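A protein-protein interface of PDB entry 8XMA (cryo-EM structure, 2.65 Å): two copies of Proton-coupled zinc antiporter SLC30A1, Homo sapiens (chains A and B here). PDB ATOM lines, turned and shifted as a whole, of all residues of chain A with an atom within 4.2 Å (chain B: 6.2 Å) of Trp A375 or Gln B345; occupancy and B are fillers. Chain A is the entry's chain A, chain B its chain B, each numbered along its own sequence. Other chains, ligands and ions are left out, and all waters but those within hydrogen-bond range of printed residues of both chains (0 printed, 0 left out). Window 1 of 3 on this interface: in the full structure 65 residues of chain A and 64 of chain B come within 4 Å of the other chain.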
ATOM      1  N   ASN A  70      22.615   2.331  11.325  1.00  0.00           N
ATOM      2  CA  ASN A  70      23.334   1.074  11.518  1.00  0.00           C
ATOM      3  C   ASN A  70      24.080   0.740  10.234  1.00  0.00           C
ATOM      4  O   ASN A  70      23.455   0.495   9.199  1.00  0.00           O
ATOM      5  CB  ASN A  70      22.373  -0.050  11.905  1.00  0.00           C
ATOM      6  CG  ASN A  70      23.087  -1.324  12.296  1.00  0.00           C
ATOM      7  OD1 ASN A  70      24.310  -1.407  12.236  1.00  0.00           O
ATOM      8  ND2 ASN A  70      22.323  -2.327  12.710  1.00  0.00           N
ATOM      9  N   PHE A  72      25.881  -1.930   9.658  1.00  0.00           N
ATOM     10  CA  PHE A  72      25.794  -3.351   9.357  1.00  0.00           C
ATOM     11  C   PHE A  72      24.415  -3.765   8.873  1.00  0.00           C
ATOM     12  O   PHE A  72      24.228  -4.926   8.497  1.00  0.00           O
ATOM     13  CB  PHE A  72      26.158  -4.179  10.594  1.00  0.00           C
ATOM     14  CG  PHE A  72      27.626  -4.207  10.897  1.00  0.00           C
ATOM     15  CD1 PHE A  72      28.473  -5.051  10.204  1.00  0.00           C
ATOM     16  CD2 PHE A  72      28.158  -3.396  11.880  1.00  0.00           C
ATOM     17  CE1 PHE A  72      29.821  -5.084  10.485  1.00  0.00           C
ATOM     18  CE2 PHE A  72      29.505  -3.424  12.165  1.00  0.00           C
ATOM     19  CZ  PHE A  72      30.338  -4.268  11.466  1.00  0.00           C
ATOM     20  N   ARG A  76      20.901  -8.330  12.523  1.00  0.00           N
ATOM     21  CA  ARG A  76      20.946  -8.896  13.863  1.00  0.00           C
ATOM     22  C   ARG A  76      19.589  -8.841  14.558  1.00  0.00           C
ATOM     23  O   ARG A  76      19.448  -9.380  15.661  1.00  0.00           O
ATOM     24  CB  ARG A  76      22.013  -8.164  14.689  1.00  0.00           C
ATOM     25  CG  ARG A  76      22.328  -8.782  16.040  1.00  0.00           C
ATOM     26  CD  ARG A  76      23.633  -8.268  16.617  1.00  0.00           C
ATOM     27  NE  ARG A  76      24.754  -9.147  16.307  1.00  0.00           N
ATOM     28  CZ  ARG A  76      25.955  -9.046  16.857  1.00  0.00           C
ATOM     29  NH1 ARG A  76      26.228  -8.111  17.750  1.00  0.00           N
ATOM     30  NH2 ARG A  76      26.903  -9.909  16.507  1.00  0.00           N
ATOM     31  N   GLN A 345      29.487 -10.869  21.181  1.00  0.00           N
ATOM     32  CA  GLN A 345      30.649 -10.868  20.291  1.00  0.00           C
ATOM     33  C   GLN A 345      31.497 -12.126  20.453  1.00  0.00           C
ATOM     34  O   GLN A 345      32.696 -12.116  20.166  1.00  0.00           O
ATOM     35  CB  GLN A 345      31.510  -9.618  20.497  1.00  0.00           C
ATOM     36  CG  GLN A 345      30.727  -8.322  20.487  1.00  0.00           C
ATOM     37  CD  GLN A 345      30.218  -7.969  19.111  1.00  0.00           C
ATOM     38  OE1 GLN A 345      29.079  -7.538  18.950  1.00  0.00           O
ATOM     39  NE2 GLN A 345      31.060  -8.153  18.108  1.00  0.00           N
ATOM     40  N   VAL A 374      37.751 -11.485  16.278  1.00  0.00           N
ATOM     41  CA  VAL A 374      36.865 -12.314  15.471  1.00  0.00           C
ATOM     42  C   VAL A 374      35.520 -12.393  16.177  1.00  0.00           C
ATOM     43  O   VAL A 374      35.462 -12.702  17.372  1.00  0.00           O
ATOM     44  CB  VAL A 374      37.439 -13.725  15.248  1.00  0.00           C
ATOM     45  CG1 VAL A 374      36.477 -14.566  14.430  1.00  0.00           C
ATOM     46  CG2 VAL A 374      38.796 -13.649  14.572  1.00  0.00           C
ATOM     47  N   TRP A 375      34.445 -12.114  15.445  1.00  0.00           N
ATOM     48  CA  TRP A 375      33.110 -12.167  16.019  1.00  0.00           C
ATOM     49  C   TRP A 375      32.108 -12.514  14.931  1.00  0.00           C
ATOM     50  O   TRP A 375      32.383 -12.379  13.737  1.00  0.00           O
ATOM     51  CB  TRP A 375      32.732 -10.848  16.704  1.00  0.00           C
ATOM     52  CG  TRP A 375      32.905  -9.630  15.851  1.00  0.00           C
ATOM     53  CD1 TRP A 375      34.073  -8.987  15.568  1.00  0.00           C
ATOM     54  CD2 TRP A 375      31.872  -8.895  15.186  1.00  0.00           C
ATOM     55  NE1 TRP A 375      33.834  -7.904  14.761  1.00  0.00           N
ATOM     56  CE2 TRP A 375      32.489  -7.826  14.512  1.00  0.00           C
ATOM     57  CE3 TRP A 375      30.487  -9.042  15.092  1.00  0.00           C
ATOM     58  CZ2 TRP A 375      31.768  -6.909  13.756  1.00  0.00           C
ATOM     59  CZ3 TRP A 375      29.775  -8.131  14.341  1.00  0.00           C
ATOM     60  CH2 TRP A 375      30.414  -7.079  13.684  1.00  0.00           C
ATOM     61  N   GLN A 376      30.937 -12.970  15.363  1.00  0.00           N
ATOM     62  CA  GLN A 376      29.867 -13.380  14.465  1.00  0.00           C
ATOM     63  C   GLN A 376      28.772 -12.324  14.460  1.00  0.00           C
ATOM     64  O   GLN A 376      28.296 -11.913  15.523  1.00  0.00           O
ATOM     65  CB  GLN A 376      29.294 -14.732  14.892  1.00  0.00           C
ATOM     66  CG  GLN A 376      28.154 -15.230  14.030  1.00  0.00           C
ATOM     67  CD  GLN A 376      27.559 -16.517  14.555  1.00  0.00           C
ATOM     68  OE1 GLN A 376      27.971 -17.026  15.595  1.00  0.00           O
ATOM     69  NE2 GLN A 376      26.581 -17.052  13.837  1.00  0.00           N
ATOM     70  N   LEU A 377      28.376 -11.888  13.266  1.00  0.00           N
ATOM     71  CA  LEU A 377      27.319 -10.890  13.154  1.00  0.00           C
ATOM     72  C   LEU A 377      25.945 -11.533  13.291  1.00  0.00           C
ATOM     73  O   LEU A 377      25.183 -11.210  14.207  1.00  0.00           O
ATOM     74  CB  LEU A 377      27.437 -10.150  11.820  1.00  0.00           C
ATOM     75  CG  LEU A 377      26.478  -8.987  11.576  1.00  0.00           C
ATOM     76  CD1 LEU A 377      26.378  -8.096  12.799  1.00  0.00           C
ATOM     77  CD2 LEU A 377      26.935  -8.189  10.375  1.00  0.00           C
ATOM     78  N   ILE A 382      30.751 -13.870   9.589  1.00  0.00           N
ATOM     79  CA  ILE A 382      31.792 -13.728  10.600  1.00  0.00           C
ATOM     80  C   ILE A 382      32.785 -12.679  10.125  1.00  0.00           C
ATOM     81  O   ILE A 382      33.260 -12.736   8.984  1.00  0.00           O
ATOM     82  CB  ILE A 382      32.493 -15.070  10.873  1.00  0.00           C
ATOM     83  CG1 ILE A 382      31.476 -16.106  11.349  1.00  0.00           C
ATOM     84  CG2 ILE A 382      33.587 -14.896  11.905  1.00  0.00           C
ATOM     85  CD1 ILE A 382      31.922 -17.531  11.154  1.00  0.00           C
ATOM     86  N   ILE A 383      33.098 -11.724  10.997  1.00  0.00           N
ATOM     87  CA  ILE A 383      34.002 -10.623  10.688  1.00  0.00           C
ATOM     88  C   ILE A 383      35.256 -10.777  11.534  1.00  0.00           C
ATOM     89  O   ILE A 383      35.171 -10.945  12.755  1.00  0.00           O
ATOM     90  CB  ILE A 383      33.337  -9.259  10.939  1.00  0.00           C
ATOM     91  CG1 ILE A 383      32.060  -9.129  10.112  1.00  0.00           C
ATOM     92  CG2 ILE A 383      34.297  -8.130  10.612  1.00  0.00           C
ATOM     93  CD1 ILE A 383      30.803  -9.320  10.910  1.00  0.00           C
ATOM     94  N   THR B  71      37.231 -12.702  21.940  1.00  0.00           N
ATOM     95  CA  THR B  71      38.411 -11.878  21.700  1.00  0.00           C
ATOM     96  C   THR B  71      38.302 -10.502  22.342  1.00  0.00           C
ATOM     97  O   THR B  71      39.323  -9.923  22.727  1.00  0.00           O
ATOM     98  CB  THR B  71      38.651 -11.728  20.199  1.00  0.00           C
ATOM     99  OG1 THR B  71      37.448 -11.278  19.567  1.00  0.00           O
ATOM    100  CG2 THR B  71      39.056 -13.058  19.600  1.00  0.00           C
ATOM    101  N   PHE B  72      37.092  -9.958  22.456  1.00  0.00           N
ATOM    102  CA  PHE B  72      36.911  -8.645  23.059  1.00  0.00           C
ATOM    103  C   PHE B  72      36.871  -8.686  24.579  1.00  0.00           C
ATOM    104  O   PHE B  72      36.856  -7.623  25.204  1.00  0.00           O
ATOM    105  CB  PHE B  72      35.620  -7.996  22.556  1.00  0.00           C
ATOM    106  CG  PHE B  72      35.615  -7.708  21.086  1.00  0.00           C
ATOM    107  CD1 PHE B  72      36.133  -6.522  20.600  1.00  0.00           C
ATOM    108  CD2 PHE B  72      35.082  -8.617  20.191  1.00  0.00           C
ATOM    109  CE1 PHE B  72      36.126  -6.252  19.250  1.00  0.00           C
ATOM    110  CE2 PHE B  72      35.073  -8.351  18.841  1.00  0.00           C
ATOM    111  CZ  PHE B  72      35.596  -7.166  18.369  1.00  0.00           C
ATOM    112  N   ARG B  76      30.962  -6.503  27.194  1.00  0.00           N
ATOM    113  CA  ARG B  76      29.550  -6.363  26.869  1.00  0.00           C
ATOM    114  C   ARG B  76      28.640  -7.064  27.869  1.00  0.00           C
ATOM    115  O   ARG B  76      27.448  -7.227  27.592  1.00  0.00           O
ATOM    116  CB  ARG B  76      29.274  -6.889  25.462  1.00  0.00           C
ATOM    117  CG  ARG B  76      29.228  -5.800  24.416  1.00  0.00           C
ATOM    118  CD  ARG B  76      28.610  -6.283  23.124  1.00  0.00           C
ATOM    119  NE  ARG B  76      28.456  -5.195  22.169  1.00  0.00           N
ATOM    120  CZ  ARG B  76      27.967  -5.337  20.946  1.00  0.00           C
ATOM    121  NH1 ARG B  76      27.570  -6.515  20.495  1.00  0.00           N
ATOM    122  NH2 ARG B  76      27.871  -4.272  20.158  1.00  0.00           N
ATOM    123  N   ALA B 340      19.273  -2.264  23.667  1.00  0.00           N
ATOM    124  CA  ALA B 340      19.049  -3.023  22.442  1.00  0.00           C
ATOM    125  C   ALA B 340      19.825  -2.431  21.275  1.00  0.00           C
ATOM    126  O   ALA B 340      20.368  -3.169  20.446  1.00  0.00           O
ATOM    127  CB  ALA B 340      17.558  -3.082  22.124  1.00  0.00           C
ATOM    128  N   LEU B 341      19.894  -1.101  21.190  1.00  0.00           N
ATOM    129  CA  LEU B 341      20.648  -0.476  20.114  1.00  0.00           C
ATOM    130  C   LEU B 341      22.149  -0.647  20.287  1.00  0.00           C
ATOM    131  O   LEU B 341      22.883  -0.559  19.299  1.00  0.00           O
ATOM    132  CB  LEU B 341      20.302   1.009  20.017  1.00  0.00           C
ATOM    133  CG  LEU B 341      18.923   1.347  19.448  1.00  0.00           C
ATOM    134  CD1 LEU B 341      18.873   2.795  18.995  1.00  0.00           C
ATOM    135  CD2 LEU B 341      18.558   0.411  18.309  1.00  0.00           C
ATOM    136  N   ILE B 342      22.628  -0.859  21.513  1.00  0.00           N
ATOM    137  CA  ILE B 342      24.042  -1.172  21.696  1.00  0.00           C
ATOM    138  C   ILE B 342      24.335  -2.614  21.298  1.00  0.00           C
ATOM    139  O   ILE B 342      25.345  -2.890  20.642  1.00  0.00           O
ATOM    140  CB  ILE B 342      24.478  -0.881  23.142  1.00  0.00           C
ATOM    141  CG1 ILE B 342      24.478   0.625  23.402  1.00  0.00           C
ATOM    142  CG2 ILE B 342      25.860  -1.447  23.403  1.00  0.00           C
ATOM    143  CD1 ILE B 342      25.060   1.013  24.739  1.00  0.00           C
ATOM    144  N   LEU B 343      23.469  -3.557  21.688  1.00  0.00           N
ATOM    145  CA  LEU B 343      23.693  -4.951  21.308  1.00  0.00           C
ATOM    146  C   LEU B 343      23.654  -5.123  19.795  1.00  0.00           C
ATOM    147  O   LEU B 343      24.489  -5.832  19.223  1.00  0.00           O
ATOM    148  CB  LEU B 343      22.677  -5.878  21.974  1.00  0.00           C
ATOM    149  CG  LEU B 343      22.934  -6.356  23.408  1.00  0.00           C
ATOM    150  CD1 LEU B 343      24.189  -7.204  23.465  1.00  0.00           C
ATOM    151  CD2 LEU B 343      23.021  -5.241  24.402  1.00  0.00           C
ATOM    152  N   LEU B 344      22.686  -4.498  19.132  1.00  0.00           N
ATOM    153  CA  LEU B 344      22.775  -4.341  17.690  1.00  0.00           C
ATOM    154  C   LEU B 344      23.935  -3.408  17.366  1.00  0.00           C
ATOM    155  O   LEU B 344      24.264  -2.506  18.136  1.00  0.00           O
ATOM    156  CB  LEU B 344      21.467  -3.789  17.124  1.00  0.00           C
ATOM    157  CG  LEU B 344      20.198  -4.583  17.439  1.00  0.00           C
ATOM    158  CD1 LEU B 344      18.987  -3.670  17.470  1.00  0.00           C
ATOM    159  CD2 LEU B 344      19.995  -5.697  16.433  1.00  0.00           C
ATOM    160  N   GLN B 345      24.571  -3.634  16.220  1.00  0.00           N
ATOM    161  CA  GLN B 345      25.802  -2.916  15.897  1.00  0.00           C
ATOM    162  C   GLN B 345      25.496  -1.527  15.328  1.00  0.00           C
ATOM    163  O   GLN B 345      26.012  -1.112  14.292  1.00  0.00           O
ATOM    164  CB  GLN B 345      26.646  -3.741  14.936  1.00  0.00           C
ATOM    165  CG  GLN B 345      26.898  -5.157  15.409  1.00  0.00           C
ATOM    166  CD  GLN B 345      27.891  -5.218  16.546  1.00  0.00           C
ATOM    167  OE1 GLN B 345      27.570  -4.881  17.684  1.00  0.00           O
ATOM    168  NE2 GLN B 345      29.106  -5.649  16.245  1.00  0.00           N
ATOM    169  N   THR B 346      24.660  -0.793  16.057  1.00  0.00           N
ATOM    170  CA  THR B 346      24.236   0.530  15.624  1.00  0.00           C
ATOM    171  C   THR B 346      25.340   1.550  15.845  1.00  0.00           C
ATOM    172  O   THR B 346      26.091   1.476  16.822  1.00  0.00           O
ATOM    173  CB  THR B 346      22.981   0.968  16.377  1.00  0.00           C
ATOM    174  OG1 THR B 346      23.278   1.070  17.773  1.00  0.00           O
ATOM    175  CG2 THR B 346      21.869  -0.039  16.180  1.00  0.00           C
ATOM    176  N   VAL B 347      25.433   2.508  14.927  1.00  0.00           N
ATOM    177  CA  VAL B 347      26.393   3.604  15.092  1.00  0.00           C
ATOM    178  C   VAL B 347      25.997   4.426  16.309  1.00  0.00           C
ATOM    179  O   VAL B 347      24.798   4.719  16.493  1.00  0.00           O
ATOM    180  CB  VAL B 347      26.435   4.475  13.826  1.00  0.00           C
ATOM    181  CG1 VAL B 347      27.394   5.636  14.002  1.00  0.00           C
ATOM    182  CG2 VAL B 347      26.824   3.637  12.627  1.00  0.00           C
ATOM    183  N   VAL B 374      31.148   1.299  11.744  1.00  0.00           N
ATOM    184  CA  VAL B 374      31.330   1.929  13.044  1.00  0.00           C
ATOM    185  C   VAL B 374      30.288   1.359  13.994  1.00  0.00           C
ATOM    186  O   VAL B 374      29.093   1.359  13.682  1.00  0.00           O
ATOM    187  CB  VAL B 374      31.211   3.461  12.958  1.00  0.00           C
ATOM    188  CG1 VAL B 374      31.266   4.075  14.345  1.00  0.00           C
ATOM    189  CG2 VAL B 374      32.311   4.027  12.080  1.00  0.00           C
ATOM    190  N   TRP B 375      30.740   0.871  15.145  1.00  0.00           N
ATOM    191  CA  TRP B 375      29.832   0.312  16.134  1.00  0.00           C
ATOM    192  C   TRP B 375      30.416   0.520  17.520  1.00  0.00           C
ATOM    193  O   TRP B 375      31.606   0.801  17.682  1.00  0.00           O
ATOM    194  CB  TRP B 375      29.556  -1.175  15.879  1.00  0.00           C
ATOM    195  CG  TRP B 375      30.781  -2.017  15.730  1.00  0.00           C
ATOM    196  CD1 TRP B 375      31.601  -2.085  14.644  1.00  0.00           C
ATOM    197  CD2 TRP B 375      31.315  -2.930  16.694  1.00  0.00           C
ATOM    198  NE1 TRP B 375      32.617  -2.977  14.874  1.00  0.00           N
ATOM    199  CE2 TRP B 375      32.464  -3.510  16.126  1.00  0.00           C
ATOM    200  CE3 TRP B 375      30.936  -3.310  17.983  1.00  0.00           C
ATOM    201  CZ2 TRP B 375      33.236  -4.447  16.803  1.00  0.00           C
ATOM    202  CZ3 TRP B 375      31.704  -4.240  18.651  1.00  0.00           C
ATOM    203  CH2 TRP B 375      32.840  -4.798  18.062  1.00  0.00           C
ATOM    204  N   GLN B 376      29.556   0.383  18.522  1.00  0.00           N
ATOM    205  CA  GLN B 376      29.909   0.620  19.914  1.00  0.00           C
ATOM    206  C   GLN B 376      29.966  -0.707  20.654  1.00  0.00           C
ATOM    207  O   GLN B 376      29.016  -1.494  20.597  1.00  0.00           O
ATOM    208  CB  GLN B 376      28.892   1.551  20.575  1.00  0.00           C
ATOM    209  CG  GLN B 376      29.221   1.943  21.997  1.00  0.00           C
ATOM    210  CD  GLN B 376      28.136   2.793  22.620  1.00  0.00           C
ATOM    211  OE1 GLN B 376      27.076   2.994  22.030  1.00  0.00           O
ATOM    212  NE2 GLN B 376      28.394   3.301  23.817  1.00  0.00           N
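NH1 of Arg A76 lies within hydrogen-bond range of O of Leu B343. The guanidinium group of Arg A76 sits at hydrogen-bond distance from the side-chain amide oxygen of Gln B345. The side-chain amide nitrogen (NE2) of Gln B345 sits at hydrogen-bond distance from the side-chain amide oxygen (OE1) of Gln A345, 3.3 Å away. The guanidinium group of Arg A76 lies close to the guanidinium group of Arg B76, at 3.4 Å. OE1 of Gln A345 sits close to NH1 of Arg B76. The backbone carbonyl oxygen (O) of Val A374 lies within hydrogen-bond range of the side-chain hydroxyl (OG1) of Thr B71 (3.3 Å). O of Gln B345 sits close to OD1 of Asn A70 (2.7 Å).
O of Gln A376 is in hydrogen-bond range of NH2 of Arg A76, 2.6 Å away. The guanidinium group of Arg A76 sits at hydrogen-bond distance from the backbone carbonyl oxygen of Leu A377, 3.0 Å away. O of Gln B376 sits at hydrogen-bond distance from NH2 of Arg B76 (3.0 Å). N of Phe A72 is in hydrogen-bond range of OD1 of Asn A70, at 3.1 Å. The guanidinium group of Arg A76 is in hydrogen-bond range of the side-chain amide oxygen of Gln A345 (3.1 Å). The backbone carbonyl oxygen (O) of Trp A375 is in hydrogen-bond range of the backbone NH (N) of Ile A383 (2.9 Å).
Among the printed residues, pairs that only touch across the chains: Asn A70 with Thr B346, Phe A72 with Gln B345, Phe A72 with Trp B375, Arg A76 with Leu B344, Gln A345 with Phe B72, Gln A345 with Trp B375, Trp A375 with Phe B72, Trp A375 with Gln B345 and Leu A377 with Gln B345.
Printed residues of chain B within 4 Å of Phe A72: Gln B345 (3.4 Å) and Trp B375 (3.5 Å). Of the printed residues of chain B, Gln A345 touches Phe B72 (3.7 Å), Arg B76 (2.4 Å), Gln B345 (3.3 Å) and Trp B375 (3.8 Å). Of the printed residues of chain B, Trp A375 touches Phe B72 and Gln B345. Of the printed residues of chain A, Thr B71 touches Val A374. Of the printed residues of chain A, Phe B72 touches Gln A345 and Trp A375. Of the printed residues of chain A, Leu B343 touches Arg A76 (3.2 Å). Of chain A, only Asn A70, Phe A72, Arg A76, Gln A345, Trp A375 and Leu A377 come within 4 Å of Gln B345. Val B374 touches none of the printed residues of chain A. Gln B376 touches none of the printed residues of chain A. The nearest residue of chain B that does not touch Trp A375 is Trp B375 (4.1 Å). The nearest printed residue of chain A that does not touch Gln B345 is Gln A376 (6.4 Å).
Of the 10 printed residues of chain A, 7 touch a printed residue of chain B. Hydrophobic or aromatic side chains of chain A that line the printed part of chain B: Phe A72, Trp A375 and Leu A377. Among the printed residues, no Asp or Glu carboxylate lies within 4 Å of a Lys or Arg side-chain nitrogen of the other chain.
Phe A72 touches Gln B345, and with the chains exchanged Gln A345 touches Phe B72. Phe A72 touches Trp B375, and with the chains exchanged Trp A375 touches Phe B72. Gln A345 touches its own counterpart, Gln B345. Gln A345 touches Trp B375, and with the chains exchanged Trp A375 touches Gln B345. Positions printed for both chains: 72, 76, 345, 374, 375 and 376.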
